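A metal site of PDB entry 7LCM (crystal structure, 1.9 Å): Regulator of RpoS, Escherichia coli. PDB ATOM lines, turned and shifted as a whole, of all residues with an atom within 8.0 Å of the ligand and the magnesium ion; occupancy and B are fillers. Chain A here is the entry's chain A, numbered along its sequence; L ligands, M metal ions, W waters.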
ATOM      1  N   VAL A  16      -9.171  26.371   4.313  1.00  0.00           N
ATOM      2  CA  VAL A  16      -9.553  25.216   5.153  1.00  0.00           C
ATOM      3  C   VAL A  16     -10.833  24.623   4.554  1.00  0.00           C
ATOM      4  O   VAL A  16     -11.877  25.274   4.559  1.00  0.00           O
ATOM      5  CB  VAL A  16      -9.764  25.608   6.621  1.00  0.00           C
ATOM      6  CG1 VAL A  16      -9.937  24.368   7.490  1.00  0.00           C
ATOM      7  CG2 VAL A  16      -8.592  26.453   7.155  1.00  0.00           C
ATOM      8  N   GLU A  17     -10.768  23.377   4.074  1.00  0.00           N
ATOM      9  CA  GLU A  17     -11.823  22.822   3.233  1.00  0.00           C
ATOM     10  C   GLU A  17     -11.641  21.314   3.121  1.00  0.00           C
ATOM     11  O   GLU A  17     -10.548  20.873   2.739  1.00  0.00           O
ATOM     12  CB  GLU A  17     -11.773  23.486   1.848  1.00  0.00           C
ATOM     13  CG  GLU A  17     -12.518  22.763   0.748  1.00  0.00           C
ATOM     14  CD  GLU A  17     -14.014  22.724   0.973  1.00  0.00           C
ATOM     15  OE1 GLU A  17     -14.641  23.797   1.146  1.00  0.00           O
ATOM     16  OE2 GLU A  17     -14.556  21.604   1.014  1.00  0.00           O
ATOM     17  N   ASP A  18     -12.684  20.534   3.415  1.00  0.00           N
ATOM     18  CA  ASP A  18     -12.500  19.080   3.455  1.00  0.00           C
ATOM     19  C   ASP A  18     -12.646  18.394   2.103  1.00  0.00           C
ATOM     20  O   ASP A  18     -12.207  17.238   1.967  1.00  0.00           O
ATOM     21  CB  ASP A  18     -13.483  18.427   4.440  1.00  0.00           C
ATOM     22  CG  ASP A  18     -14.950  18.646   4.056  1.00  0.00           C
ATOM     23  OD1 ASP A  18     -15.384  19.801   3.841  1.00  0.00           O
ATOM     24  OD2 ASP A  18     -15.662  17.634   3.955  1.00  0.00           O
ATOM     25  N   GLU A  19     -13.262  19.022   1.111  1.00  0.00           N
ATOM     26  CA  GLU A  19     -13.417  18.392  -0.198  1.00  0.00           C
ATOM     27  C   GLU A  19     -12.189  18.730  -1.033  1.00  0.00           C
ATOM     28  O   GLU A  19     -11.925  19.902  -1.299  1.00  0.00           O
ATOM     29  CB  GLU A  19     -14.694  18.831  -0.910  1.00  0.00           C
ATOM     30  CG  GLU A  19     -15.980  18.467  -0.179  1.00  0.00           C
ATOM     31  CD  GLU A  19     -17.239  18.968  -0.884  1.00  0.00           C
ATOM     32  OE1 GLU A  19     -17.250  19.036  -2.140  1.00  0.00           O
ATOM     33  OE2 GLU A  19     -18.204  19.332  -0.172  1.00  0.00           O
ATOM     34  N   PHE A  22     -12.557  21.000  -4.198  1.00  0.00           N
ATOM     35  CA  PHE A  22     -12.697  22.441  -3.981  1.00  0.00           C
ATOM     36  C   PHE A  22     -11.406  23.032  -3.432  1.00  0.00           C
ATOM     37  O   PHE A  22     -11.021  24.154  -3.791  1.00  0.00           O
ATOM     38  CB  PHE A  22     -13.875  22.712  -3.061  1.00  0.00           C
ATOM     39  CG  PHE A  22     -14.381  24.114  -3.163  1.00  0.00           C
ATOM     40  CD1 PHE A  22     -14.815  24.603  -4.370  1.00  0.00           C
ATOM     41  CD2 PHE A  22     -14.399  24.940  -2.056  1.00  0.00           C
ATOM     42  CE1 PHE A  22     -15.271  25.894  -4.471  1.00  0.00           C
ATOM     43  CE2 PHE A  22     -14.838  26.237  -2.166  1.00  0.00           C
ATOM     44  CZ  PHE A  22     -15.268  26.705  -3.379  1.00  0.00           C
ATOM     45  N   ALA A  41      -6.884  20.299   4.990  1.00  0.00           N
ATOM     46  CA  ALA A  41      -8.108  19.548   4.754  1.00  0.00           C
ATOM     47  C   ALA A  41      -9.008  19.495   5.972  1.00  0.00           C
ATOM     48  O   ALA A  41     -10.196  19.187   5.845  1.00  0.00           O
ATOM     49  CB  ALA A  41      -7.739  18.125   4.290  1.00  0.00           C
ATOM     50  N   CYS A  60     -12.563  29.616   4.693  1.00  0.00           N
ATOM     51  CA  CYS A  60     -12.977  28.555   5.598  1.00  0.00           C
ATOM     52  C   CYS A  60     -14.331  28.001   5.198  1.00  0.00           C
ATOM     53  O   CYS A  60     -15.270  28.746   4.926  1.00  0.00           O
ATOM     54  CB  CYS A  60     -13.044  29.055   7.029  1.00  0.00           C
ATOM     55  SG  CYS A  60     -13.189  27.676   8.153  1.00  0.00           S
ATOM     56  N   ASP A  61     -14.424  26.682   5.224  1.00  0.00           N
ATOM     57  CA  ASP A  61     -15.632  25.900   5.024  1.00  0.00           C
ATOM     58  C   ASP A  61     -16.355  25.760   6.363  1.00  0.00           C
ATOM     59  O   ASP A  61     -15.779  25.985   7.427  1.00  0.00           O
ATOM     60  CB  ASP A  61     -15.218  24.546   4.463  1.00  0.00           C
ATOM     61  CG  ASP A  61     -16.343  23.703   4.045  1.00  0.00           C
ATOM     62  OD1 ASP A  61     -17.369  24.273   3.626  1.00  0.00           O
ATOM     63  OD2 ASP A  61     -16.200  22.469   4.147  1.00  0.00           O
ATOM     64  N   ILE A  62     -17.635  25.393   6.316  1.00  0.00           N
ATOM     65  CA  ILE A  62     -18.333  25.166   7.581  1.00  0.00           C
ATOM     66  C   ILE A  62     -18.399  23.674   7.861  1.00  0.00           C
ATOM     67  O   ILE A  62     -17.810  23.219   8.846  1.00  0.00           O
ATOM     68  CB  ILE A  62     -19.713  25.823   7.601  1.00  0.00           C
ATOM     69  CG1 ILE A  62     -19.550  27.337   7.678  1.00  0.00           C
ATOM     70  CG2 ILE A  62     -20.498  25.395   8.840  1.00  0.00           C
ATOM     71  CD1 ILE A  62     -20.898  28.080   7.590  1.00  0.00           C
ATOM     72  N   ALA A  63     -19.051  22.879   7.003  1.00  0.00           N
ATOM     73  CA  ALA A  63     -19.192  21.456   7.295  1.00  0.00           C
ATOM     74  C   ALA A  63     -17.902  20.721   6.965  1.00  0.00           C
ATOM     75  O   ALA A  63     -17.488  20.639   5.812  1.00  0.00           O
ATOM     76  CB  ALA A  63     -20.378  20.867   6.520  1.00  0.00           C
ATOM     77  N   MET A  64     -17.239  20.193   7.997  1.00  0.00           N
ATOM     78  CA  MET A  64     -16.022  19.401   7.872  1.00  0.00           C
ATOM     79  C   MET A  64     -16.040  18.304   8.926  1.00  0.00           C
ATOM     80  O   MET A  64     -16.582  18.499  10.019  1.00  0.00           O
ATOM     81  CB  MET A  64     -14.757  20.255   8.026  1.00  0.00           C
ATOM     82  CG  MET A  64     -14.775  21.607   7.271  1.00  0.00           C
ATOM     83  SD  MET A  64     -13.161  22.373   7.248  1.00  0.00           S
ATOM     84  CE  MET A  64     -13.353  23.322   8.752  1.00  0.00           C
ATOM     85  N   PRO A  65     -15.425  17.132   8.619  1.00  0.00           N
ATOM     86  CA  PRO A  65     -15.671  15.905   9.402  1.00  0.00           C
ATOM     87  C   PRO A  65     -15.489  15.962  10.908  1.00  0.00           C
ATOM     88  O   PRO A  65     -16.426  15.646  11.659  1.00  0.00           O
ATOM     89  CB  PRO A  65     -14.669  14.907   8.800  1.00  0.00           C
ATOM     90  CG  PRO A  65     -14.417  15.408   7.447  1.00  0.00           C
ATOM     91  CD  PRO A  65     -14.463  16.891   7.532  1.00  0.00           C
ATOM     92  N   ASN A  68     -16.047  21.322  12.730  1.00  0.00           N
ATOM     93  CA  ASN A  68     -16.568  22.202  11.700  1.00  0.00           C
ATOM     94  C   ASN A  68     -15.940  23.585  11.813  1.00  0.00           C
ATOM     95  O   ASN A  68     -15.267  23.915  12.793  1.00  0.00           O
ATOM     96  CB  ASN A  68     -18.103  22.270  11.784  1.00  0.00           C
ATOM     97  CG  ASN A  68     -18.607  22.962  13.048  1.00  0.00           C
ATOM     98  OD1 ASN A  68     -18.388  24.164  13.231  1.00  0.00           O
ATOM     99  ND2 ASN A  68     -19.288  22.219  13.899  1.00  0.00           N
ATOM    100  N   GLY A  69     -16.148  24.396  10.774  1.00  0.00           N
ATOM    101  CA  GLY A  69     -15.510  25.694  10.717  1.00  0.00           C
ATOM    102  C   GLY A  69     -16.015  26.671  11.758  1.00  0.00           C
ATOM    103  O   GLY A  69     -15.290  27.605  12.126  1.00  0.00           O
ATOM    104  N   VAL A  87     -15.910  33.025   4.610  1.00  0.00           N
ATOM    105  CA  VAL A  87     -16.479  31.688   4.661  1.00  0.00           C
ATOM    106  C   VAL A  87     -17.088  31.378   3.299  1.00  0.00           C
ATOM    107  O   VAL A  87     -17.843  32.181   2.740  1.00  0.00           O
ATOM    108  CB  VAL A  87     -17.519  31.565   5.790  1.00  0.00           C
ATOM    109  CG1 VAL A  87     -18.168  30.175   5.767  1.00  0.00           C
ATOM    110  CG2 VAL A  87     -16.877  31.866   7.141  1.00  0.00           C
ATOM    111  N   ILE A  88     -16.744  30.216   2.754  1.00  0.00           N
ATOM    112  CA  ILE A  88     -17.370  29.709   1.526  1.00  0.00           C
ATOM    113  C   ILE A  88     -17.974  28.366   1.887  1.00  0.00           C
ATOM    114  O   ILE A  88     -17.248  27.419   2.186  1.00  0.00           O
ATOM    115  CB  ILE A  88     -16.400  29.579   0.346  1.00  0.00           C
ATOM    116  CG1 ILE A  88     -15.732  30.922   0.038  1.00  0.00           C
ATOM    117  CG2 ILE A  88     -17.138  29.051  -0.862  1.00  0.00           C
ATOM    118  CD1 ILE A  88     -14.718  30.859  -1.103  1.00  0.00           C
ATOM    119  N   SER A  89     -19.300  28.287   1.849  1.00  0.00           N
ATOM    120  CA  SER A  89     -20.024  27.131   2.350  1.00  0.00           C
ATOM    121  C   SER A  89     -21.263  26.871   1.508  1.00  0.00           C
ATOM    122  O   SER A  89     -21.850  27.797   0.942  1.00  0.00           O
ATOM    123  CB  SER A  89     -20.446  27.339   3.816  1.00  0.00           C
ATOM    124  OG  SER A  89     -21.232  26.252   4.288  1.00  0.00           O
ATOM    125  N   ALA A  90     -21.657  25.592   1.456  1.00  0.00           N
ATOM    126  CA  ALA A  90     -22.938  25.177   0.882  1.00  0.00           C
ATOM    127  C   ALA A  90     -24.102  25.308   1.851  1.00  0.00           C
ATOM    128  O   ALA A  90     -25.241  25.008   1.464  1.00  0.00           O
ATOM    129  CB  ALA A  90     -22.863  23.716   0.395  1.00  0.00           C
ATOM    130  N   THR A  91     -23.866  25.753   3.081  1.00  0.00           N
ATOM    131  CA  THR A  91     -24.929  25.766   4.077  1.00  0.00           C
ATOM    132  C   THR A  91     -26.068  26.707   3.683  1.00  0.00           C
ATOM    133  O   THR A  91     -25.849  27.787   3.114  1.00  0.00           O
ATOM    134  CB  THR A  91     -24.413  26.152   5.466  1.00  0.00           C
ATOM    135  OG1 THR A  91     -25.438  25.839   6.433  1.00  0.00           O
ATOM    136  CG2 THR A  91     -24.067  27.633   5.556  1.00  0.00           C
ATOM    137  N   GLU A  92     -27.280  26.258   3.959  1.00  0.00           N
ATOM    138  CA  GLU A  92     -28.478  27.057   3.835  1.00  0.00           C
ATOM    139  C   GLU A  92     -29.012  27.424   5.211  1.00  0.00           C
ATOM    140  O   GLU A  92     -30.023  28.135   5.318  1.00  0.00           O
ATOM    141  CB  GLU A  92     -29.524  26.270   3.017  1.00  0.00           C
ATOM    142  CG  GLU A  92     -30.155  26.958   1.788  1.00  0.00           C
ATOM    143  CD  GLU A  92     -31.176  28.060   2.084  1.00  0.00           C
ATOM    144  OE1 GLU A  92     -31.784  28.585   1.109  1.00  0.00           O
ATOM    145  OE2 GLU A  92     -31.415  28.412   3.250  1.00  0.00           O
ATOM    146  N   LEU A 109     -20.042  33.241   1.685  1.00  0.00           N
ATOM    147  CA  LEU A 109     -20.440  33.015   0.310  1.00  0.00           C
ATOM    148  C   LEU A 109     -21.004  31.617   0.129  1.00  0.00           C
ATOM    149  O   LEU A 109     -20.560  30.666   0.785  1.00  0.00           O
ATOM    150  CB  LEU A 109     -19.262  33.251  -0.641  1.00  0.00           C
ATOM    151  CG  LEU A 109     -18.527  34.537  -0.273  1.00  0.00           C
ATOM    152  CD1 LEU A 109     -17.406  34.875  -1.266  1.00  0.00           C
ATOM    153  CD2 LEU A 109     -19.601  35.616  -0.319  1.00  0.00           C
ATOM    154  N   LEU A 110     -21.986  31.499  -0.763  1.00  0.00           N
ATOM    155  CA  LEU A 110     -22.686  30.245  -0.998  1.00  0.00           C
ATOM    156  C   LEU A 110     -22.020  29.464  -2.122  1.00  0.00           C
ATOM    157  O   LEU A 110     -21.654  30.042  -3.163  1.00  0.00           O
ATOM    158  CB  LEU A 110     -24.158  30.523  -1.331  1.00  0.00           C
ATOM    159  CG  LEU A 110     -25.063  29.356  -1.675  1.00  0.00           C
ATOM    160  CD1 LEU A 110     -25.453  28.626  -0.397  1.00  0.00           C
ATOM    161  CD2 LEU A 110     -26.296  29.851  -2.423  1.00  0.00           C
ATOM    162  N   LYS A 111     -21.831  28.154  -1.914  1.00  0.00           N
ATOM    163  CA  LYS A 111     -21.392  27.267  -2.977  1.00  0.00           C
ATOM    164  C   LYS A 111     -22.569  26.834  -3.837  1.00  0.00           C
ATOM    165  O   LYS A 111     -23.700  26.740  -3.355  1.00  0.00           O
ATOM    166  CB  LYS A 111     -20.751  26.007  -2.390  1.00  0.00           C
ATOM    167  CG  LYS A 111     -19.474  26.210  -1.602  1.00  0.00           C
ATOM    168  CD  LYS A 111     -19.059  24.867  -1.029  1.00  0.00           C
ATOM    169  CE  LYS A 111     -17.670  24.922  -0.391  1.00  0.00           C
ATOM    170  NZ  LYS A 111     -17.321  23.600   0.227  1.00  0.00           N
HETATM  171 BE1  LIG L   1     -19.123  23.352   3.576  1.00  0.00          BE
HETATM  172  F1  LIG L   1     -19.485  23.723   2.160  1.00  0.00           F
HETATM  173  F2  LIG L   1     -18.864  21.856   3.732  1.00  0.00           F
HETATM  174  F3  LIG L   1     -20.049  23.963   4.635  1.00  0.00           F
HETATM  175 MG    MG M   1     -17.242  20.751   3.769  1.00  0.00          MG
HETATM  176  O   HOH W   1     -18.229  19.100   3.562  1.00  0.00           O
HETATM  177  O   HOH W   2     -17.051  20.973   1.739  1.00  0.00           O
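The side-chain carboxylate (OD1) of Asp 61 is bound to a beryllium atom (BE1) of the ligand. F3 of the ligand sits at hydrogen-bond distance from N of Ala 63 (2.8 Å). OG of Ser 89 lies within hydrogen-bond range of F3 of the ligand (2.6 Å). F1 of the ligand sits at hydrogen-bond distance from NZ of Lys 111, 2.9 Å away. N of Ala 90 sits at hydrogen-bond distance from F1 of the ligand. The backbone NH (N) of Ile 62 is in hydrogen-bond range of a fluorine (F3) of the ligand (3.3 Å).
The side-chain carboxylate (OD1) of Asp 61 lies close to the side-chain amino group (NZ) of Lys 111, at 3.5 Å. N of Asp 61 lies within hydrogen-bond range of O of Val 16 (3.0 Å). The backbone NH (N) of Lys 111 lies within hydrogen-bond range of the backbone carbonyl oxygen (O) of Ser 89 (2.9 Å). The backbone NH (N) of Thr 91 lies within hydrogen-bond range of the side-chain hydroxyl (OG) of Ser 89 (2.9 Å). N of Ser 89 lies within hydrogen-bond range of O of Leu 109 (2.9 Å). NZ of Lys 111 lies within salt-bridge range of OE1 of Glu 17. O of Ile 62 sits at hydrogen-bond distance from N of Gly 69, 2.8 Å away. The side-chain carboxylate (OE2) of Glu 17 sits at hydrogen-bond distance from the backbone NH (N) of Glu 19 (2.9 Å).
Hydrophobic or aromatic side chains within 4 Å of the ligand: Ile 62, Ala 63 and Ala 90. Within 4 Å of the ligand: Asp 61, Ile 62, Ala 63, Ser 89, Ala 90 and Lys 111. Along chain A the residues within 4 Å of the ligand span positions 61 to 111.
Residues that only touch the magnesium ion: Glu 17 (3.9 Å). Within 4 Å of the magnesium ion: Glu 17, Asp 18, Asp 61 and Ala 63. The nearest printed residue that does not touch the magnesium ion is Met 64 (4.3 Å).
The magnesium ion is bound by water W1 (1.9 Å), F2 of the ligand (2.0 Å), OD2 of Asp 61 (2.0 Å), water W2 (2.1 Å), O of Ala 63 (2.1 Å) and OD1 of Asp 18 (2.1 Å).
Water W2 lies within hydrogen-bond range of the side-chain carboxylate of Glu 17, the side-chain carboxylate of Glu 19 and the side-chain amino group of Lys 111.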
